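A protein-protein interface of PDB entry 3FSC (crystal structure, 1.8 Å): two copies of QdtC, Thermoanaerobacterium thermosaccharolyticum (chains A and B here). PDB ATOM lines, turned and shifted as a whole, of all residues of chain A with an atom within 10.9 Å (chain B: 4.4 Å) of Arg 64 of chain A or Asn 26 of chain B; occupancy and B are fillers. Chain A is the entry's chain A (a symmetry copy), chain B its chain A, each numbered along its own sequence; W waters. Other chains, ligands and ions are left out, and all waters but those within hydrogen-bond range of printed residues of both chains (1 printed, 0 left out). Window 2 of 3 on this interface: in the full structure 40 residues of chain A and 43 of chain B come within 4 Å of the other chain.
NH2 of Arg 64 of chain A lies within hydrogen-bond range of O of Ser 45 of chain B (3.3 Å). The backbone carbonyl oxygen of Gly 44 of chain B lies within hydrogen-bond range of the guanidinium group of Arg 64 of chain A, 2.6 Å away. The backbone carbonyl oxygen (O) of Asn 26 of chain B is in hydrogen-bond range of the guanidinium group (NH1) of Arg 64 of chain A, at 2.9 Å.
The side-chain hydroxyl of Ser 8 of chain B lies within hydrogen-bond range of the backbone NH of Asn 26 of chain B, at 3.0 Å. N of Gly 44 of chain B sits at hydrogen-bond distance from O of Asp 25 of chain B. The backbone carbonyl oxygen (O) of Ser 45 of chain B is in hydrogen-bond range of the backbone NH (N) of Tyr 28 of chain B, 2.8 Å away. N of Ile 65 of chain A sits at hydrogen-bond distance from O of Phe 60 of chain A, at 3.3 Å.
Among the printed residues, merely in contact across the chains: Arg 64 of chain A with Tyr 28 of chain B, Phe 60 of chain A with Phe 46 of chain B, Tyr 61 of chain A with Phe 46 of chain B, Arg 64 of chain A with Phe 46 of chain B and Arg 64 of chain A with Val 27 of chain B.
Tyr 56 of chain A touches none of the printed residues of chain B. Of the printed residues of chain B, Tyr 61 of chain A touches Phe 46. Of the printed residues of chain B, Arg 64 of chain A touches Asn 26 (2.9 Å), Val 27 (3.99 Å), Tyr 28 (3.4 Å), Gly 44 (2.6 Å), Ser 45 (3.3 Å) and Phe 46 (3.9 Å). No residue of chain A comes within 4 Å of Ala 9 of chain B. Asp 25 of chain B touches none of the printed residues of chain A. Of the printed residues of chain A, Asn 26 of chain B touches Arg 64. Printed residues of chain A within 4 Å of Val 27 of chain B: Arg 64. Tyr 28 of chain B touches one residue of chain A. Of chain A, only Arg 64 comes within 4 Å of Gly 44 of chain B. Of the printed residues of chain A, Phe 46 of chain B touches Phe 60 (3.8 Å), Tyr 61 (3.8 Å) and Arg 64 (3.9 Å). The nearest printed residue of chain B that does not touch Arg 64 of chain A is Ser 8 of chain B (6.1 Å).
Hydrophobic or aromatic side chains of chain A that line the printed part of chain B: Phe 60 and Tyr 61. Among the printed residues, no Asp or Glu carboxylate lies within 4 Å of a Lys or Arg side-chain nitrogen of the other chain.
No position is printed for both chains. Of the 8 pairs that touch across the chains among the printed residues, none has its exchanged pair printed and touching as well.
Water W1 bridges OH of Tyr 28 of chain B (2.7 Å) and OH of Tyr 56 of chain A (2.8 Å).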
ATOM      1  N   ARG A  36      10.349 -12.668   5.190  1.00  0.00           N
ATOM      2  CA  ARG A  36       8.957 -13.052   5.046  1.00  0.00           C
ATOM      3  C   ARG A  36       8.605 -13.943   6.250  1.00  0.00           C
ATOM      4  O   ARG A  36       9.455 -14.282   7.084  1.00  0.00           O
ATOM      5  CB  ARG A  36       8.689 -13.752   3.687  1.00  0.00           C
ATOM      6  CG  ARG A  36       9.299 -13.013   2.511  1.00  0.00           C
ATOM      7  CD  ARG A  36       8.558 -13.450   1.265  1.00  0.00           C
ATOM      8  NE  ARG A  36       8.999 -12.972  -0.044  1.00  0.00           N
ATOM      9  CZ  ARG A  36       8.674 -11.833  -0.654  1.00  0.00           C
ATOM     10  NH1 ARG A  36       9.158 -11.644  -1.878  1.00  0.00           N
ATOM     11  NH2 ARG A  36       7.923 -10.874  -0.096  1.00  0.00           N
ATOM     12  N   ASP A  37       7.338 -14.331   6.346  1.00  0.00           N
ATOM     13  CA  ASP A  37       6.862 -15.145   7.463  1.00  0.00           C
ATOM     14  C   ASP A  37       7.561 -16.460   7.658  1.00  0.00           C
ATOM     15  O   ASP A  37       8.066 -17.049   6.706  1.00  0.00           O
ATOM     16  CB  ASP A  37       5.382 -15.511   7.321  1.00  0.00           C
ATOM     17  CG  ASP A  37       4.488 -14.314   7.001  1.00  0.00           C
ATOM     18  OD1 ASP A  37       4.795 -13.175   7.447  1.00  0.00           O
ATOM     19  OD2 ASP A  37       3.461 -14.506   6.296  1.00  0.00           O
ATOM     20  N   TYR A  56       8.406 -16.919  -1.080  1.00  0.00           N
ATOM     21  CA  TYR A  56       7.209 -17.677  -1.434  1.00  0.00           C
ATOM     22  C   TYR A  56       7.283 -18.955  -2.312  1.00  0.00           C
ATOM     23  O   TYR A  56       7.786 -18.966  -3.452  1.00  0.00           O
ATOM     24  CB  TYR A  56       6.274 -16.739  -2.193  1.00  0.00           C
ATOM     25  CG  TYR A  56       5.893 -15.469  -1.482  1.00  0.00           C
ATOM     26  CD1 TYR A  56       5.419 -15.505  -0.167  1.00  0.00           C
ATOM     27  CD2 TYR A  56       5.977 -14.262  -2.130  1.00  0.00           C
ATOM     28  CE1 TYR A  56       5.013 -14.365   0.477  1.00  0.00           C
ATOM     29  CE2 TYR A  56       5.550 -13.095  -1.507  1.00  0.00           C
ATOM     30  CZ  TYR A  56       5.080 -13.173  -0.200  1.00  0.00           C
ATOM     31  OH  TYR A  56       4.716 -12.001   0.396  1.00  0.00           O
ATOM     32  N   LEU A  57       6.690 -20.026  -1.797  1.00  0.00           N
ATOM     33  CA  LEU A  57       6.574 -21.274  -2.531  1.00  0.00           C
ATOM     34  C   LEU A  57       5.415 -20.984  -3.480  1.00  0.00           C
ATOM     35  O   LEU A  57       4.681 -19.989  -3.352  1.00  0.00           O
ATOM     36  CB  LEU A  57       6.256 -22.420  -1.590  1.00  0.00           C
ATOM     37  CG  LEU A  57       7.542 -23.023  -0.995  1.00  0.00           C
ATOM     38  CD1 LEU A  57       8.338 -22.041  -0.120  1.00  0.00           C
ATOM     39  CD2 LEU A  57       7.241 -24.280  -0.150  1.00  0.00           C
ATOM     40  N   VAL A  58       5.270 -21.884  -4.440  1.00  0.00           N
ATOM     41  CA  VAL A  58       4.284 -21.801  -5.494  1.00  0.00           C
ATOM     42  C   VAL A  58       2.857 -21.647  -5.039  1.00  0.00           C
ATOM     43  O   VAL A  58       2.074 -20.901  -5.633  1.00  0.00           O
ATOM     44  CB  VAL A  58       4.444 -22.949  -6.544  1.00  0.00           C
ATOM     45  CG1 VAL A  58       3.310 -23.967  -6.405  1.00  0.00           C
ATOM     46  CG2 VAL A  58       4.459 -22.345  -7.922  1.00  0.00           C
ATOM     47  N   ASP A  59       2.526 -22.363  -3.982  1.00  0.00           N
ATOM     48  CA  ASP A  59       1.182 -22.254  -3.445  1.00  0.00           C
ATOM     49  C   ASP A  59       0.733 -20.854  -3.030  1.00  0.00           C
ATOM     50  O   ASP A  59      -0.444 -20.588  -2.903  1.00  0.00           O
ATOM     51  CB  ASP A  59       1.060 -23.219  -2.264  1.00  0.00           C
ATOM     52  CG  ASP A  59       1.980 -22.920  -1.113  1.00  0.00           C
ATOM     53  OD1 ASP A  59       2.922 -22.110  -1.220  1.00  0.00           O
ATOM     54  OD2 ASP A  59       1.772 -23.572  -0.071  1.00  0.00           O
ATOM     55  N   PHE A  60       1.662 -19.940  -2.794  1.00  0.00           N
ATOM     56  CA  PHE A  60       1.254 -18.617  -2.355  1.00  0.00           C
ATOM     57  C   PHE A  60       0.476 -17.963  -3.463  1.00  0.00           C
ATOM     58  O   PHE A  60      -0.510 -17.254  -3.260  1.00  0.00           O
ATOM     59  CB  PHE A  60       2.525 -17.772  -2.121  1.00  0.00           C
ATOM     60  CG  PHE A  60       2.262 -16.280  -2.036  1.00  0.00           C
ATOM     61  CD1 PHE A  60       1.750 -15.705  -0.874  1.00  0.00           C
ATOM     62  CD2 PHE A  60       2.520 -15.438  -3.111  1.00  0.00           C
ATOM     63  CE1 PHE A  60       1.468 -14.341  -0.801  1.00  0.00           C
ATOM     64  CE2 PHE A  60       2.238 -14.059  -3.044  1.00  0.00           C
ATOM     65  CZ  PHE A  60       1.726 -13.503  -1.876  1.00  0.00           C
ATOM     66  N   TYR A  61       0.996 -18.164  -4.668  1.00  0.00           N
ATOM     67  CA  TYR A  61       0.398 -17.537  -5.840  1.00  0.00           C
ATOM     68  C   TYR A  61      -1.017 -17.908  -6.235  1.00  0.00           C
ATOM     69  O   TYR A  61      -1.594 -17.223  -7.065  1.00  0.00           O
ATOM     70  CB  TYR A  61       1.350 -17.500  -7.047  1.00  0.00           C
ATOM     71  CG  TYR A  61       2.732 -16.989  -6.689  1.00  0.00           C
ATOM     72  CD1 TYR A  61       3.016 -15.627  -6.751  1.00  0.00           C
ATOM     73  CD2 TYR A  61       3.751 -17.867  -6.247  1.00  0.00           C
ATOM     74  CE1 TYR A  61       4.274 -15.120  -6.388  1.00  0.00           C
ATOM     75  CE2 TYR A  61       5.031 -17.354  -5.905  1.00  0.00           C
ATOM     76  CZ  TYR A  61       5.285 -15.978  -5.998  1.00  0.00           C
ATOM     77  OH  TYR A  61       6.502 -15.385  -5.692  1.00  0.00           O
ATOM     78  N   ASN A  62      -1.558 -18.975  -5.653  1.00  0.00           N
ATOM     79  CA  ASN A  62      -2.912 -19.446  -5.953  1.00  0.00           C
ATOM     80  C   ASN A  62      -3.934 -18.359  -5.645  1.00  0.00           C
ATOM     81  O   ASN A  62      -4.857 -18.068  -6.418  1.00  0.00           O
ATOM     82  CB  ASN A  62      -3.225 -20.608  -5.003  1.00  0.00           C
ATOM     83  CG  ASN A  62      -2.465 -21.867  -5.347  1.00  0.00           C
ATOM     84  OD1 ASN A  62      -2.199 -22.122  -6.527  1.00  0.00           O
ATOM     85  ND2 ASN A  62      -2.136 -22.670  -4.326  1.00  0.00           N
ATOM     86  N   ASP A  63      -3.739 -17.775  -4.472  1.00  0.00           N
ATOM     87  CA  ASP A  63      -4.636 -16.739  -3.988  1.00  0.00           C
ATOM     88  C   ASP A  63      -3.899 -15.648  -3.243  1.00  0.00           C
ATOM     89  O   ASP A  63      -4.521 -14.883  -2.524  1.00  0.00           O
ATOM     90  CB  ASP A  63      -5.542 -17.406  -2.963  1.00  0.00           C
ATOM     91  CG  ASP A  63      -4.777 -18.208  -1.921  1.00  0.00           C
ATOM     92  OD1 ASP A  63      -3.536 -18.181  -1.852  1.00  0.00           O
ATOM     93  OD2 ASP A  63      -5.450 -18.891  -1.123  1.00  0.00           O
ATOM     94  N   ARG A  64      -2.583 -15.580  -3.385  1.00  0.00           N
ATOM     95  CA  ARG A  64      -1.827 -14.558  -2.686  1.00  0.00           C
ATOM     96  C   ARG A  64      -1.956 -14.612  -1.198  1.00  0.00           C
ATOM     97  O   ARG A  64      -1.852 -13.574  -0.535  1.00  0.00           O
ATOM     98  CB  ARG A  64      -1.997 -13.151  -3.243  1.00  0.00           C
ATOM     99  CG  ARG A  64      -1.359 -13.043  -4.602  1.00  0.00           C
ATOM    100  CD  ARG A  64      -1.795 -11.794  -5.353  1.00  0.00           C
ATOM    101  NE  ARG A  64      -1.555 -11.877  -6.800  1.00  0.00           N
ATOM    102  CZ  ARG A  64      -1.984 -11.001  -7.714  1.00  0.00           C
ATOM    103  NH1 ARG A  64      -2.700  -9.941  -7.350  1.00  0.00           N
ATOM    104  NH2 ARG A  64      -1.676 -11.182  -9.007  1.00  0.00           N
ATOM    105  N   ILE A  65      -2.121 -15.835  -0.689  1.00  0.00           N
ATOM    106  CA  ILE A  65      -2.191 -15.990   0.751  1.00  0.00           C
ATOM    107  C   ILE A  65      -1.008 -16.878   1.023  1.00  0.00           C
ATOM    108  O   ILE A  65      -0.904 -17.991   0.471  1.00  0.00           O
ATOM    109  CB  ILE A  65      -3.410 -16.758   1.231  1.00  0.00           C
ATOM    110  CG1 ILE A  65      -4.623 -15.816   1.276  1.00  0.00           C
ATOM    111  CG2 ILE A  65      -3.101 -17.294   2.613  1.00  0.00           C
ATOM    112  CD1 ILE A  65      -5.878 -16.395   0.671  1.00  0.00           C
ATOM    113  N   ASN A  66      -0.118 -16.331   1.845  1.00  0.00           N
ATOM    114  CA  ASN A  66       1.107 -17.005   2.240  1.00  0.00           C
ATOM    115  C   ASN A  66       0.898 -18.104   3.278  1.00  0.00           C
ATOM    116  O   ASN A  66       0.512 -17.838   4.420  1.00  0.00           O
ATOM    117  CB  ASN A  66       2.160 -15.988   2.724  1.00  0.00           C
ATOM    118  CG  ASN A  66       3.532 -16.644   2.966  1.00  0.00           C
ATOM    119  OD1 ASN A  66       3.816 -17.691   2.359  1.00  0.00           O
ATOM    120  ND2 ASN A  66       4.378 -16.051   3.828  1.00  0.00           N
ATOM    121  N   LYS A  67       1.148 -19.343   2.857  1.00  0.00           N
ATOM    122  CA  LYS A  67       1.077 -20.507   3.730  1.00  0.00           C
ATOM    123  C   LYS A  67       2.356 -20.699   4.541  1.00  0.00           C
ATOM    124  O   LYS A  67       3.439 -20.079   4.360  1.00  0.00           O
ATOM    125  CB  LYS A  67       0.705 -21.782   3.005  1.00  0.00           C
ATOM    126  CG  LYS A  67      -0.740 -21.765   2.410  1.00  0.00           C
ATOM    127  CD  LYS A  67      -1.053 -20.633   1.457  1.00  0.00           C
ATOM    128  CE  LYS A  67      -1.067 -21.027  -0.012  1.00  0.00           C
ATOM    129  NZ  LYS A  67      -1.881 -19.938  -0.656  1.00  0.00           N
ATOM    130  N   LYS A  68       2.220 -21.596   5.497  1.00  0.00           N
ATOM    131  CA  LYS A  68       3.311 -21.843   6.401  1.00  0.00           C
ATOM    132  C   LYS A  68       4.370 -22.810   5.948  1.00  0.00           C
ATOM    133  O   LYS A  68       4.128 -24.018   5.884  1.00  0.00           O
ATOM    134  CB  LYS A  68       2.727 -22.279   7.736  1.00  0.00           C
ATOM    135  CG  LYS A  68       3.603 -22.011   8.953  1.00  0.00           C
ATOM    136  CD  LYS A  68       3.162 -22.919  10.125  1.00  0.00           C
ATOM    137  CE  LYS A  68       4.258 -23.244  11.153  1.00  0.00           C
ATOM    138  NZ  LYS A  68       3.823 -23.135  12.590  1.00  0.00           N
ATOM    139  N   SER B   8      -7.863  -1.973  -7.308  1.00  0.00           N
ATOM    140  CA  SER B   8      -7.639  -3.369  -6.884  1.00  0.00           C
ATOM    141  C   SER B   8      -6.155  -3.741  -6.946  1.00  0.00           C
ATOM    142  O   SER B   8      -5.729  -4.736  -6.384  1.00  0.00           O
ATOM    143  CB  SER B   8      -8.482  -4.377  -7.653  1.00  0.00           C
ATOM    144  OG  SER B   8      -8.252  -4.317  -9.047  1.00  0.00           O
ATOM    145  N   ALA B   9      -5.341  -2.925  -7.595  1.00  0.00           N
ATOM    146  CA  ALA B   9      -3.925  -3.237  -7.591  1.00  0.00           C
ATOM    147  C   ALA B   9      -3.394  -3.133  -6.153  1.00  0.00           C
ATOM    148  O   ALA B   9      -3.820  -2.260  -5.393  1.00  0.00           O
ATOM    149  CB  ALA B   9      -3.209  -2.230  -8.454  1.00  0.00           C
ATOM    150  N   GLU B  24      -3.080  -2.464 -14.316  1.00  0.00           N
ATOM    151  CA  GLU B  24      -4.422  -2.970 -14.295  1.00  0.00           C
ATOM    152  C   GLU B  24      -4.881  -3.603 -12.984  1.00  0.00           C
ATOM    153  O   GLU B  24      -4.216  -3.660 -11.936  1.00  0.00           O
ATOM    154  CB  GLU B  24      -4.651  -3.868 -15.511  1.00  0.00           C
ATOM    155  CG  GLU B  24      -4.405  -3.127 -16.838  1.00  0.00           C
ATOM    156  CD  GLU B  24      -4.733  -3.975 -18.062  1.00  0.00           C
ATOM    157  OE1 GLU B  24      -4.665  -3.427 -19.178  1.00  0.00           O
ATOM    158  OE2 GLU B  24      -5.054  -5.178 -17.965  1.00  0.00           O
ATOM    159  N   ASP B  25      -6.106  -4.068 -13.102  1.00  0.00           N
ATOM    160  CA  ASP B  25      -6.783  -4.713 -12.019  1.00  0.00           C
ATOM    161  C   ASP B  25      -6.083  -5.931 -11.469  1.00  0.00           C
ATOM    162  O   ASP B  25      -5.664  -6.797 -12.240  1.00  0.00           O
ATOM    163  CB  ASP B  25      -8.078  -5.246 -12.606  1.00  0.00           C
ATOM    164  CG  ASP B  25      -9.141  -4.166 -12.715  1.00  0.00           C
ATOM    165  OD1 ASP B  25      -8.872  -3.013 -12.264  1.00  0.00           O
ATOM    166  OD2 ASP B  25     -10.227  -4.516 -13.254  1.00  0.00           O
ATOM    167  N   ASN B  26      -6.055  -5.966 -10.136  1.00  0.00           N
ATOM    168  CA  ASN B  26      -5.508  -7.090  -9.367  1.00  0.00           C
ATOM    169  C   ASN B  26      -4.089  -7.426  -9.689  1.00  0.00           C
ATOM    170  O   ASN B  26      -3.735  -8.606  -9.745  1.00  0.00           O
ATOM    171  CB  ASN B  26      -6.214  -8.369  -9.787  1.00  0.00           C
ATOM    172  CG  ASN B  26      -7.716  -8.208  -9.761  1.00  0.00           C
ATOM    173  OD1 ASN B  26      -8.251  -7.798  -8.751  1.00  0.00           O
ATOM    174  ND2 ASN B  26      -8.389  -8.495 -10.871  1.00  0.00           N
ATOM    175  N   VAL B  27      -3.289  -6.396  -9.893  1.00  0.00           N
ATOM    176  CA  VAL B  27      -1.890  -6.617 -10.177  1.00  0.00           C
ATOM    177  C   VAL B  27      -1.347  -6.461  -8.768  1.00  0.00           C
ATOM    178  O   VAL B  27      -1.870  -5.715  -7.939  1.00  0.00           O
ATOM    179  CB  VAL B  27      -1.400  -5.436 -11.009  1.00  0.00           C
ATOM    180  CG1 VAL B  27       0.089  -5.207 -10.813  1.00  0.00           C
ATOM    181  CG2 VAL B  27      -1.842  -5.682 -12.460  1.00  0.00           C
ATOM    182  N   TYR B  28      -0.256  -7.148  -8.484  1.00  0.00           N
ATOM    183  CA  TYR B  28       0.313  -7.014  -7.164  1.00  0.00           C
ATOM    184  C   TYR B  28       1.769  -6.703  -7.430  1.00  0.00           C
ATOM    185  O   TYR B  28       2.437  -7.462  -8.114  1.00  0.00           O
ATOM    186  CB  TYR B  28       0.179  -8.382  -6.512  1.00  0.00           C
ATOM    187  CG  TYR B  28       0.672  -8.454  -5.100  1.00  0.00           C
ATOM    188  CD1 TYR B  28      -0.215  -8.727  -4.068  1.00  0.00           C
ATOM    189  CD2 TYR B  28       2.010  -8.266  -4.793  1.00  0.00           C
ATOM    190  CE1 TYR B  28       0.221  -8.813  -2.765  1.00  0.00           C
ATOM    191  CE2 TYR B  28       2.466  -8.366  -3.484  1.00  0.00           C
ATOM    192  CZ  TYR B  28       1.565  -8.635  -2.465  1.00  0.00           C
ATOM    193  OH  TYR B  28       1.980  -8.738  -1.149  1.00  0.00           O
ATOM    194  N   GLY B  44      -4.140  -8.941 -13.247  1.00  0.00           N
ATOM    195  CA  GLY B  44      -3.857 -10.169 -12.519  1.00  0.00           C
ATOM    196  C   GLY B  44      -2.370 -10.466 -12.296  1.00  0.00           C
ATOM    197  O   GLY B  44      -2.035 -11.426 -11.608  1.00  0.00           O
ATOM    198  N   SER B  45      -1.486  -9.671 -12.890  1.00  0.00           N
ATOM    199  CA  SER B  45      -0.056  -9.935 -12.743  1.00  0.00           C
ATOM    200  C   SER B  45       0.526  -9.715 -11.372  1.00  0.00           C
ATOM    201  O   SER B  45       0.036  -8.894 -10.602  1.00  0.00           O
ATOM    202  CB  SER B  45       0.725  -9.140 -13.765  1.00  0.00           C
ATOM    203  OG  SER B  45       0.274  -9.565 -15.045  1.00  0.00           O
ATOM    204  N   PHE B  46       1.570 -10.498 -11.105  1.00  0.00           N
ATOM    205  CA  PHE B  46       2.329 -10.405  -9.859  1.00  0.00           C
ATOM    206  C   PHE B  46       3.733  -9.930 -10.275  1.00  0.00           C
ATOM    207  O   PHE B  46       4.375 -10.495 -11.179  1.00  0.00           O
ATOM    208  CB  PHE B  46       2.451 -11.739  -9.104  1.00  0.00           C
ATOM    209  CG  PHE B  46       3.297 -11.635  -7.869  1.00  0.00           C
ATOM    210  CD1 PHE B  46       2.708 -11.518  -6.619  1.00  0.00           C
ATOM    211  CD2 PHE B  46       4.685 -11.654  -7.950  1.00  0.00           C
ATOM    212  CE1 PHE B  46       3.458 -11.443  -5.459  1.00  0.00           C
ATOM    213  CE2 PHE B  46       5.462 -11.550  -6.801  1.00  0.00           C
ATOM    214  CZ  PHE B  46       4.851 -11.448  -5.549  1.00  0.00           C
HETATM  215  O   HOH W   1       4.456  -9.235  -0.152  1.00  0.00           O
